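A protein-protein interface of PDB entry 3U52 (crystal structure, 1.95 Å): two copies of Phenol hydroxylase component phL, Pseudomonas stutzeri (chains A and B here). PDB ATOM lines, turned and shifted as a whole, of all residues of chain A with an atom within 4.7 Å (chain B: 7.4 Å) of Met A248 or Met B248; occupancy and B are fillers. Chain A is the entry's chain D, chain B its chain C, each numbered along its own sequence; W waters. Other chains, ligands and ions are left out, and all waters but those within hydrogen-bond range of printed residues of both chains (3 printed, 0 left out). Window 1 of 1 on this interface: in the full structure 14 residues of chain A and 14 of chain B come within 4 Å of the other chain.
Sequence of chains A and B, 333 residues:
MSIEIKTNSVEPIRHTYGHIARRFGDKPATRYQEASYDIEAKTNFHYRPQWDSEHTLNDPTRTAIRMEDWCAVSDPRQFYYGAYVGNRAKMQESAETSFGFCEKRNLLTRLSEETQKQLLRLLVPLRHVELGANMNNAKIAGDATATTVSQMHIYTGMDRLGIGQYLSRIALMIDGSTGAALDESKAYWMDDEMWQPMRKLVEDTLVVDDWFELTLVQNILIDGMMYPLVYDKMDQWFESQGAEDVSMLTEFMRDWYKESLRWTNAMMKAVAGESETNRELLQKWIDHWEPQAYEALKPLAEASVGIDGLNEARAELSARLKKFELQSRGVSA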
ATOM      1  N   SER A  98      -9.760  -6.725 -16.612  1.00  0.00           N
ATOM      2  CA  SER A  98     -10.739  -7.825 -16.821  1.00  0.00           C
ATOM      3  C   SER A  98     -10.066  -9.138 -17.186  1.00  0.00           C
ATOM      4  O   SER A  98     -10.468 -10.174 -16.711  1.00  0.00           O
ATOM      5  CB  SER A  98     -11.774  -7.441 -17.850  1.00  0.00           C
ATOM      6  OG  SER A  98     -12.459  -6.318 -17.363  1.00  0.00           O
ATOM      7  N   PHE A 101      -8.390 -10.542 -13.928  1.00  0.00           N
ATOM      8  CA  PHE A 101      -9.480 -11.077 -13.102  1.00  0.00           C
ATOM      9  C   PHE A 101      -9.950 -12.473 -13.580  1.00  0.00           C
ATOM     10  O   PHE A 101     -10.130 -13.364 -12.781  1.00  0.00           O
ATOM     11  CB  PHE A 101     -10.605 -10.059 -13.175  1.00  0.00           C
ATOM     12  CG  PHE A 101     -11.798 -10.363 -12.334  1.00  0.00           C
ATOM     13  CD1 PHE A 101     -11.860  -9.928 -10.999  1.00  0.00           C
ATOM     14  CD2 PHE A 101     -12.905 -10.990 -12.886  1.00  0.00           C
ATOM     15  CE1 PHE A 101     -13.007 -10.153 -10.235  1.00  0.00           C
ATOM     16  CE2 PHE A 101     -14.043 -11.231 -12.127  1.00  0.00           C
ATOM     17  CZ  PHE A 101     -14.102 -10.803 -10.814  1.00  0.00           C
ATOM     18  N   CYS A 102     -10.138 -12.662 -14.889  1.00  0.00           N
ATOM     19  CA  CYS A 102     -10.574 -13.959 -15.418  1.00  0.00           C
ATOM     20  C   CYS A 102      -9.459 -14.999 -15.269  1.00  0.00           C
ATOM     21  O   CYS A 102      -9.721 -16.143 -14.925  1.00  0.00           O
ATOM     22  CB  CYS A 102     -11.032 -13.835 -16.870  1.00  0.00           C
ATOM     23  SG  CYS A 102     -12.524 -12.808 -17.079  1.00  0.00           S
ATOM     24  N   LEU A 107     -11.826 -18.292 -14.621  1.00  0.00           N
ATOM     25  CA  LEU A 107     -13.167 -18.219 -15.161  1.00  0.00           C
ATOM     26  C   LEU A 107     -13.313 -18.989 -16.488  1.00  0.00           C
ATOM     27  O   LEU A 107     -14.383 -19.510 -16.778  1.00  0.00           O
ATOM     28  CB  LEU A 107     -13.620 -16.755 -15.273  1.00  0.00           C
ATOM     29  CG  LEU A 107     -13.643 -16.004 -13.922  1.00  0.00           C
ATOM     30  CD1 LEU A 107     -14.236 -14.601 -14.062  1.00  0.00           C
ATOM     31  CD2 LEU A 107     -14.459 -16.796 -12.885  1.00  0.00           C
ATOM     32  N   ASP A 245     -19.128 -15.508 -18.751  1.00  0.00           N
ATOM     33  CA  ASP A 245     -17.949 -14.733 -18.317  1.00  0.00           C
ATOM     34  C   ASP A 245     -17.068 -14.157 -19.452  1.00  0.00           C
ATOM     35  O   ASP A 245     -16.400 -13.169 -19.258  1.00  0.00           O
ATOM     36  CB  ASP A 245     -17.120 -15.516 -17.288  1.00  0.00           C
ATOM     37  CG  ASP A 245     -17.901 -15.755 -15.954  1.00  0.00           C
ATOM     38  OD1 ASP A 245     -18.971 -15.149 -15.762  1.00  0.00           O
ATOM     39  OD2 ASP A 245     -17.438 -16.545 -15.096  1.00  0.00           O
ATOM     40  N   VAL A 246     -17.099 -14.732 -20.644  1.00  0.00           N
ATOM     41  CA  VAL A 246     -16.364 -14.122 -21.774  1.00  0.00           C
ATOM     42  C   VAL A 246     -16.881 -12.737 -22.170  1.00  0.00           C
ATOM     43  O   VAL A 246     -16.180 -12.023 -22.840  1.00  0.00           O
ATOM     44  CB  VAL A 246     -16.306 -15.019 -23.060  1.00  0.00           C
ATOM     45  CG1 VAL A 246     -15.890 -16.430 -22.705  1.00  0.00           C
ATOM     46  CG2 VAL A 246     -17.625 -15.000 -23.762  1.00  0.00           C
ATOM     47  N   SER A 247     -18.088 -12.360 -21.758  1.00  0.00           N
ATOM     48  CA  SER A 247     -18.624 -11.011 -21.994  1.00  0.00           C
ATOM     49  C   SER A 247     -17.741  -9.882 -21.458  1.00  0.00           C
ATOM     50  O   SER A 247     -17.709  -8.795 -22.008  1.00  0.00           O
ATOM     51  CB  SER A 247     -19.979 -10.838 -21.327  1.00  0.00           C
ATOM     52  OG  SER A 247     -21.009 -11.431 -22.064  1.00  0.00           O
ATOM     53  N   MET A 248     -17.086 -10.120 -20.337  1.00  0.00           N
ATOM     54  CA  MET A 248     -16.274  -9.077 -19.773  1.00  0.00           C
ATOM     55  C   MET A 248     -15.007  -8.944 -20.590  1.00  0.00           C
ATOM     56  O   MET A 248     -14.392  -7.866 -20.616  1.00  0.00           O
ATOM     57  CB  MET A 248     -15.995  -9.315 -18.275  1.00  0.00           C
ATOM     58  CG  MET A 248     -15.149 -10.538 -17.929  1.00  0.00           C
ATOM     59  SD  MET A 248     -14.943 -10.692 -16.090  1.00  0.00           S
ATOM     60  CE  MET A 248     -16.490 -11.411 -15.579  1.00  0.00           C
ATOM     61  N   LEU A 249     -14.631 -10.014 -21.289  1.00  0.00           N
ATOM     62  CA  LEU A 249     -13.448  -9.965 -22.177  1.00  0.00           C
ATOM     63  C   LEU A 249     -13.699  -9.308 -23.528  1.00  0.00           C
ATOM     64  O   LEU A 249     -12.776  -8.878 -24.190  1.00  0.00           O
ATOM     65  CB  LEU A 249     -12.831 -11.354 -22.321  1.00  0.00           C
ATOM     66  CG  LEU A 249     -12.542 -12.054 -20.984  1.00  0.00           C
ATOM     67  CD1 LEU A 249     -11.959 -13.444 -21.242  1.00  0.00           C
ATOM     68  CD2 LEU A 249     -11.556 -11.207 -20.135  1.00  0.00           C
ATOM     69  N   THR A 250     -14.953  -9.185 -23.929  1.00  0.00           N
ATOM     70  CA  THR A 250     -15.265  -8.650 -25.247  1.00  0.00           C
ATOM     71  C   THR A 250     -15.907  -7.284 -25.130  1.00  0.00           C
ATOM     72  O   THR A 250     -16.476  -6.770 -26.096  1.00  0.00           O
ATOM     73  CB  THR A 250     -16.207  -9.622 -26.003  1.00  0.00           C
ATOM     74  OG1 THR A 250     -17.336  -9.870 -25.174  1.00  0.00           O
ATOM     75  CG2 THR A 250     -15.489 -10.989 -26.274  1.00  0.00           C
ATOM     76  N   GLU A 251     -15.841  -6.673 -23.943  1.00  0.00           N
ATOM     77  CA  GLU A 251     -16.479  -5.376 -23.796  1.00  0.00           C
ATOM     78  C   GLU A 251     -15.661  -4.346 -24.591  1.00  0.00           C
ATOM     79  O   GLU A 251     -16.198  -3.403 -25.126  1.00  0.00           O
ATOM     80  CB  GLU A 251     -16.626  -4.977 -22.300  1.00  0.00           C
ATOM     81  CG  GLU A 251     -17.494  -3.696 -22.020  1.00  0.00           C
ATOM     82  CD  GLU A 251     -19.013  -3.807 -22.328  1.00  0.00           C
ATOM     83  OE1 GLU A 251     -19.570  -4.917 -22.522  1.00  0.00           O
ATOM     84  OE2 GLU A 251     -19.668  -2.748 -22.354  1.00  0.00           O
ATOM     85  N   SER B  94     -10.845   1.237 -13.747  1.00  0.00           N
ATOM     86  CA  SER B  94     -11.390  -0.136 -13.812  1.00  0.00           C
ATOM     87  C   SER B  94     -12.643  -0.338 -12.982  1.00  0.00           C
ATOM     88  O   SER B  94     -13.550  -1.055 -13.418  1.00  0.00           O
ATOM     89  CB  SER B  94     -10.376  -1.151 -13.317  1.00  0.00           C
ATOM     90  OG  SER B  94      -9.243  -1.167 -14.148  1.00  0.00           O
ATOM     91  N   ALA B  95     -12.688   0.213 -11.768  1.00  0.00           N
ATOM     92  CA  ALA B  95     -13.906   0.082 -10.972  1.00  0.00           C
ATOM     93  C   ALA B  95     -15.094   0.711 -11.662  1.00  0.00           C
ATOM     94  O   ALA B  95     -16.143   0.095 -11.699  1.00  0.00           O
ATOM     95  CB  ALA B  95     -13.745   0.652  -9.574  1.00  0.00           C
ATOM     96  N   THR B  97     -15.766   1.253 -14.845  1.00  0.00           N
ATOM     97  CA  THR B  97     -16.140   0.439 -15.993  1.00  0.00           C
ATOM     98  C   THR B  97     -16.919  -0.807 -15.535  1.00  0.00           C
ATOM     99  O   THR B  97     -17.854  -1.228 -16.188  1.00  0.00           O
ATOM    100  CB  THR B  97     -14.856   0.054 -16.776  1.00  0.00           C
ATOM    101  OG1 THR B  97     -14.493   1.177 -17.612  1.00  0.00           O
ATOM    102  CG2 THR B  97     -15.092  -1.107 -17.654  1.00  0.00           C
ATOM    103  N   SER B  98     -16.483  -1.428 -14.448  1.00  0.00           N
ATOM    104  CA  SER B  98     -17.198  -2.620 -13.901  1.00  0.00           C
ATOM    105  C   SER B  98     -18.578  -2.245 -13.357  1.00  0.00           C
ATOM    106  O   SER B  98     -19.535  -2.996 -13.518  1.00  0.00           O
ATOM    107  CB  SER B  98     -16.370  -3.289 -12.817  1.00  0.00           C
ATOM    108  OG  SER B  98     -15.201  -3.869 -13.375  1.00  0.00           O
ATOM    109  N   PHE B  99     -18.687  -1.079 -12.734  1.00  0.00           N
ATOM    110  CA  PHE B  99     -19.996  -0.553 -12.317  1.00  0.00           C
ATOM    111  C   PHE B  99     -20.921  -0.274 -13.492  1.00  0.00           C
ATOM    112  O   PHE B  99     -22.121  -0.577 -13.422  1.00  0.00           O
ATOM    113  CB  PHE B  99     -19.876   0.676 -11.372  1.00  0.00           C
ATOM    114  CG  PHE B  99     -19.704   0.296  -9.895  1.00  0.00           C
ATOM    115  CD1 PHE B  99     -18.467  -0.008  -9.370  1.00  0.00           C
ATOM    116  CD2 PHE B  99     -20.823   0.177  -9.049  1.00  0.00           C
ATOM    117  CE1 PHE B  99     -18.312  -0.414  -8.020  1.00  0.00           C
ATOM    118  CE2 PHE B  99     -20.668  -0.202  -7.684  1.00  0.00           C
ATOM    119  CZ  PHE B  99     -19.424  -0.497  -7.171  1.00  0.00           C
ATOM    120  N   PHE B 101     -20.782  -1.691 -16.568  1.00  0.00           N
ATOM    121  CA  PHE B 101     -21.047  -3.006 -17.130  1.00  0.00           C
ATOM    122  C   PHE B 101     -22.144  -3.748 -16.350  1.00  0.00           C
ATOM    123  O   PHE B 101     -23.087  -4.257 -16.968  1.00  0.00           O
ATOM    124  CB  PHE B 101     -19.744  -3.793 -17.105  1.00  0.00           C
ATOM    125  CG  PHE B 101     -19.836  -5.207 -17.632  1.00  0.00           C
ATOM    126  CD1 PHE B 101     -19.654  -5.470 -19.007  1.00  0.00           C
ATOM    127  CD2 PHE B 101     -19.998  -6.279 -16.749  1.00  0.00           C
ATOM    128  CE1 PHE B 101     -19.647  -6.798 -19.482  1.00  0.00           C
ATOM    129  CE2 PHE B 101     -20.036  -7.593 -17.209  1.00  0.00           C
ATOM    130  CZ  PHE B 101     -19.857  -7.855 -18.577  1.00  0.00           C
ATOM    131  N   CYS B 102     -22.012  -3.827 -15.029  1.00  0.00           N
ATOM    132  CA  CYS B 102     -23.028  -4.470 -14.193  1.00  0.00           C
ATOM    133  C   CYS B 102     -24.373  -3.742 -14.257  1.00  0.00           C
ATOM    134  O   CYS B 102     -25.431  -4.362 -14.280  1.00  0.00           O
ATOM    135  CB  CYS B 102     -22.590  -4.560 -12.736  1.00  0.00           C
ATOM    136  SG  CYS B 102     -21.300  -5.787 -12.402  1.00  0.00           S
ATOM    137  N   ARG B 105     -26.120  -4.298 -17.871  1.00  0.00           N
ATOM    138  CA  ARG B 105     -26.537  -5.674 -18.109  1.00  0.00           C
ATOM    139  C   ARG B 105     -27.453  -6.177 -17.010  1.00  0.00           C
ATOM    140  O   ARG B 105     -27.774  -7.395 -16.972  1.00  0.00           O
ATOM    141  CB  ARG B 105     -25.329  -6.624 -18.162  1.00  0.00           C
ATOM    142  CG  ARG B 105     -24.336  -6.280 -19.196  1.00  0.00           C
ATOM    143  CD  ARG B 105     -23.415  -7.419 -19.432  1.00  0.00           C
ATOM    144  NE  ARG B 105     -22.929  -7.220 -20.778  1.00  0.00           N
ATOM    145  CZ  ARG B 105     -22.954  -8.110 -21.756  1.00  0.00           C
ATOM    146  NH1 ARG B 105     -23.383  -9.348 -21.561  1.00  0.00           N
ATOM    147  NH2 ARG B 105     -22.499  -7.747 -22.932  1.00  0.00           N
ATOM    148  N   LEU B 107     -26.948  -6.951 -13.911  1.00  0.00           N
ATOM    149  CA  LEU B 107     -26.354  -8.049 -13.167  1.00  0.00           C
ATOM    150  C   LEU B 107     -26.765  -8.100 -11.692  1.00  0.00           C
ATOM    151  O   LEU B 107     -26.756  -9.192 -11.109  1.00  0.00           O
ATOM    152  CB  LEU B 107     -24.827  -8.076 -13.316  1.00  0.00           C
ATOM    153  CG  LEU B 107     -24.320  -8.183 -14.761  1.00  0.00           C
ATOM    154  CD1 LEU B 107     -22.801  -8.299 -14.758  1.00  0.00           C
ATOM    155  CD2 LEU B 107     -24.955  -9.399 -15.464  1.00  0.00           C
ATOM    156  N   ASP B 235     -16.422 -13.719  -0.091  1.00  0.00           N
ATOM    157  CA  ASP B 235     -16.413 -13.572  -1.535  1.00  0.00           C
ATOM    158  C   ASP B 235     -16.551 -14.912  -2.237  1.00  0.00           C
ATOM    159  O   ASP B 235     -17.365 -15.046  -3.159  1.00  0.00           O
ATOM    160  CB  ASP B 235     -15.147 -12.883  -2.045  1.00  0.00           C
ATOM    161  CG  ASP B 235     -15.251 -12.541  -3.535  1.00  0.00           C
ATOM    162  OD1 ASP B 235     -16.064 -11.644  -3.875  1.00  0.00           O
ATOM    163  OD2 ASP B 235     -14.547 -13.171  -4.367  1.00  0.00           O
ATOM    164  N   ALA B 243     -24.214 -14.970  -6.407  1.00  0.00           N
ATOM    165  CA  ALA B 243     -23.849 -13.544  -6.449  1.00  0.00           C
ATOM    166  C   ALA B 243     -22.380 -13.290  -6.916  1.00  0.00           C
ATOM    167  O   ALA B 243     -21.789 -12.249  -6.591  1.00  0.00           O
ATOM    168  CB  ALA B 243     -24.093 -12.932  -5.094  1.00  0.00           C
ATOM    169  N   GLU B 244     -21.824 -14.234  -7.663  1.00  0.00           N
ATOM    170  CA  GLU B 244     -20.448 -14.166  -8.177  1.00  0.00           C
ATOM    171  C   GLU B 244     -20.153 -12.822  -8.899  1.00  0.00           C
ATOM    172  O   GLU B 244     -19.033 -12.306  -8.852  1.00  0.00           O
ATOM    173  CB  GLU B 244     -20.247 -15.315  -9.181  1.00  0.00           C
ATOM    174  CG  GLU B 244     -21.429 -16.378  -9.188  1.00  0.00           C
ATOM    175  CD  GLU B 244     -21.804 -16.868 -10.611  1.00  0.00           C
ATOM    176  OE1 GLU B 244     -22.360 -16.065 -11.425  1.00  0.00           O
ATOM    177  OE2 GLU B 244     -21.532 -18.070 -10.904  1.00  0.00           O
ATOM    178  N   ASP B 245     -21.153 -12.264  -9.576  1.00  0.00           N
ATOM    179  CA  ASP B 245     -20.963 -11.036 -10.318  1.00  0.00           C
ATOM    180  C   ASP B 245     -20.642  -9.814  -9.439  1.00  0.00           C
ATOM    181  O   ASP B 245     -20.070  -8.848  -9.933  1.00  0.00           O
ATOM    182  CB  ASP B 245     -22.172 -10.771 -11.180  1.00  0.00           C
ATOM    183  CG  ASP B 245     -22.279 -11.776 -12.346  1.00  0.00           C
ATOM    184  OD1 ASP B 245     -21.279 -12.497 -12.619  1.00  0.00           O
ATOM    185  OD2 ASP B 245     -23.367 -11.847 -12.970  1.00  0.00           O
ATOM    186  N   VAL B 246     -20.947  -9.888  -8.140  1.00  0.00           N
ATOM    187  CA  VAL B 246     -20.592  -8.808  -7.211  1.00  0.00           C
ATOM    188  C   VAL B 246     -19.054  -8.672  -7.011  1.00  0.00           C
ATOM    189  O   VAL B 246     -18.566  -7.581  -6.713  1.00  0.00           O
ATOM    190  CB  VAL B 246     -21.304  -8.953  -5.852  1.00  0.00           C
ATOM    191  CG1 VAL B 246     -20.969  -7.765  -4.938  1.00  0.00           C
ATOM    192  CG2 VAL B 246     -22.817  -8.970  -6.083  1.00  0.00           C
ATOM    193  N   SER B 247     -18.343  -9.784  -7.179  1.00  0.00           N
ATOM    194  CA  SER B 247     -16.896  -9.846  -7.149  1.00  0.00           C
ATOM    195  C   SER B 247     -16.209  -8.839  -8.055  1.00  0.00           C
ATOM    196  O   SER B 247     -15.125  -8.339  -7.695  1.00  0.00           O
ATOM    197  CB  SER B 247     -16.407 -11.236  -7.513  1.00  0.00           C
ATOM    198  OG  SER B 247     -16.673 -12.087  -6.415  1.00  0.00           O
ATOM    199  N   MET B 248     -16.798  -8.547  -9.214  1.00  0.00           N
ATOM    200  CA  MET B 248     -16.195  -7.546 -10.049  1.00  0.00           C
ATOM    201  C   MET B 248     -16.368  -6.124  -9.521  1.00  0.00           C
ATOM    202  O   MET B 248     -15.597  -5.230  -9.891  1.00  0.00           O
ATOM    203  CB  MET B 248     -16.527  -7.690 -11.537  1.00  0.00           C
ATOM    204  CG  MET B 248     -17.939  -7.839 -11.939  1.00  0.00           C
ATOM    205  SD  MET B 248     -18.016  -8.170 -13.742  1.00  0.00           S
ATOM    206  CE  MET B 248     -19.294  -9.415 -13.790  1.00  0.00           C
ATOM    207  N   LEU B 249     -17.327  -5.928  -8.633  1.00  0.00           N
ATOM    208  CA  LEU B 249     -17.550  -4.626  -8.009  1.00  0.00           C
ATOM    209  C   LEU B 249     -16.688  -4.442  -6.744  1.00  0.00           C
ATOM    210  O   LEU B 249     -16.474  -3.303  -6.325  1.00  0.00           O
ATOM    211  CB  LEU B 249     -19.052  -4.375  -7.720  1.00  0.00           C
ATOM    212  CG  LEU B 249     -19.959  -4.563  -8.917  1.00  0.00           C
ATOM    213  CD1 LEU B 249     -21.415  -4.452  -8.495  1.00  0.00           C
ATOM    214  CD2 LEU B 249     -19.598  -3.549 -10.075  1.00  0.00           C
ATOM    215  N   THR B 250     -16.161  -5.538  -6.178  1.00  0.00           N
ATOM    216  CA  THR B 250     -15.389  -5.505  -4.936  1.00  0.00           C
ATOM    217  C   THR B 250     -13.895  -5.774  -5.166  1.00  0.00           C
ATOM    218  O   THR B 250     -13.104  -5.952  -4.204  1.00  0.00           O
ATOM    219  CB  THR B 250     -15.929  -6.538  -3.852  1.00  0.00           C
ATOM    220  OG1 THR B 250     -15.796  -7.874  -4.353  1.00  0.00           O
ATOM    221  CG2 THR B 250     -17.398  -6.300  -3.507  1.00  0.00           C
ATOM    222  N   GLU B 251     -13.488  -5.779  -6.431  1.00  0.00           N
ATOM    223  CA  GLU B 251     -12.114  -6.003  -6.765  1.00  0.00           C
ATOM    224  C   GLU B 251     -11.218  -4.862  -6.271  1.00  0.00           C
ATOM    225  O   GLU B 251     -10.071  -5.098  -5.842  1.00  0.00           O
ATOM    226  CB  GLU B 251     -11.962  -6.200  -8.269  1.00  0.00           C
ATOM    227  CG  GLU B 251     -10.624  -6.805  -8.627  1.00  0.00           C
ATOM    228  CD  GLU B 251     -10.419  -8.211  -8.025  1.00  0.00           C
ATOM    229  OE1 GLU B 251     -11.431  -8.881  -7.666  1.00  0.00           O
ATOM    230  OE2 GLU B 251      -9.234  -8.620  -7.881  1.00  0.00           O
ATOM    231  N   PHE B 252     -11.738  -3.642  -6.345  1.00  0.00           N
ATOM    232  CA  PHE B 252     -11.041  -2.440  -5.811  1.00  0.00           C
ATOM    233  C   PHE B 252     -10.618  -2.671  -4.358  1.00  0.00           C
ATOM    234  O   PHE B 252      -9.457  -2.369  -3.995  1.00  0.00           O
ATOM    235  CB  PHE B 252     -11.958  -1.201  -5.907  1.00  0.00           C
ATOM    236  CG  PHE B 252     -11.326   0.096  -5.387  1.00  0.00           C
ATOM    237  CD1 PHE B 252     -10.707   0.983  -6.266  1.00  0.00           C
ATOM    238  CD2 PHE B 252     -11.333   0.414  -4.026  1.00  0.00           C
ATOM    239  CE1 PHE B 252     -10.101   2.161  -5.804  1.00  0.00           C
ATOM    240  CE2 PHE B 252     -10.729   1.588  -3.554  1.00  0.00           C
ATOM    241  CZ  PHE B 252     -10.115   2.462  -4.446  1.00  0.00           C
ATOM    242  N   ARG B 254     -10.073  -5.583  -2.732  1.00  0.00           N
ATOM    243  CA  ARG B 254      -8.956  -6.553  -2.680  1.00  0.00           C
ATOM    244  C   ARG B 254      -7.571  -5.952  -3.064  1.00  0.00           C
ATOM    245  O   ARG B 254      -6.552  -6.214  -2.392  1.00  0.00           O
ATOM    246  CB  ARG B 254      -9.267  -7.790  -3.536  1.00  0.00           C
ATOM    247  CG  ARG B 254     -10.156  -8.821  -2.811  1.00  0.00           C
ATOM    248  CD  ARG B 254     -10.488 -10.148  -3.609  1.00  0.00           C
ATOM    249  NE  ARG B 254     -11.347  -9.780  -4.714  1.00  0.00           N
ATOM    250  CZ  ARG B 254     -12.646  -9.564  -4.637  1.00  0.00           C
ATOM    251  NH1 ARG B 254     -13.290  -9.748  -3.491  1.00  0.00           N
ATOM    252  NH2 ARG B 254     -13.294  -9.138  -5.723  1.00  0.00           N
HETATM  253  O   HOH W   1     -19.639 -16.398 -12.911  1.00  0.00           O
HETATM  254  O   HOH W   2     -22.493  -4.491 -22.495  1.00  0.00           O
HETATM  255  O   HOH W   3     -12.885  -6.391 -13.945  1.00  0.00           O
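Of the printed residues of chain B, Phe A101 touches Ser B247 (3.8 Å), Met B248 (3.9 Å) and Glu B251 (3.3 Å).
Of chain B, only Phe B101 and Met B248 come within 4 Å of Met A248.
Asp B245 touches none of the printed residues of chain A.
Val B246 touches none of the printed residues of chain A.
Of the printed residues of chain A, Ser B247 touches Phe A101.
Of the printed residues of chain A, Met B248 touches Phe A101 and Met A248.
O of Ser B247 touches CE1 of Phe A101, 3.8 Å away.
Met B248 touches Phe A101.
Phe A101 touches Glu B251 (CE1 to OE1, 3.3 Å).
Ser A247 touches Phe B101.
Met A248 touches Phe B101.
Met B248 touches Met A248 (CE to CE, 3.9 Å).
Glu A251 touches Phe B101.
The guanidinium group of Arg B105 lies within hydrogen-bond range of the side-chain hydroxyl of Ser A247.
Of the 11 printed residues of chain A, 4 touch a printed residue of chain B.
Of the 21 printed residues of chain B, 5 touch a printed residue of chain A.
Among the printed residues, no Asp or Glu carboxylate lies within 4 Å of a Lys or Arg side-chain nitrogen of the other chain.
OG of Ser B247 sits close to O of Glu B244 (3.4 Å).
The backbone carbonyl oxygen (O) of Ser B247 lies within hydrogen-bond range of the side-chain hydroxyl (OG1) of Thr B250 (3.4 Å).
The guanidinium group (NH2) of Arg B254 lies within hydrogen-bond range of the backbone carbonyl oxygen (O) of Ser B247.
The side-chain carboxylate (OE1) of Glu B251 is in salt-bridge range of the guanidinium group (NH2) of Arg B254, 2.7 Å away.
SG of Cys A102 is in hydrogen-bond range of SD of Met A248, at 3.4 Å.
O of Ser A247 sits at hydrogen-bond distance from OG1 of Thr A250, at 3.4 Å.
Phe A101 touches Ser B247, and with the chains exchanged Ser A247 touches Phe B101.
Phe A101 touches Met B248, and with the chains exchanged Met A248 touches Phe B101.
Phe A101 touches Glu B251, and with the chains exchanged Glu A251 touches Phe B101.
Met A248 touches its own counterpart, Met B248.
Positions printed for both chains: 98, 101, 102, 107, 245, 246, 247, 248, 249, 250 and 251.
Water W2 lies within hydrogen-bond range of OE1 of Glu A251 and NE of Arg B105.
Water W1 bridges OD2 of Asp A245 (3.1 Å) and OE1 of Glu B244 (3.1 Å).
Water W3 lies within hydrogen-bond range of OG of Ser A98 and OG of Ser B98.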
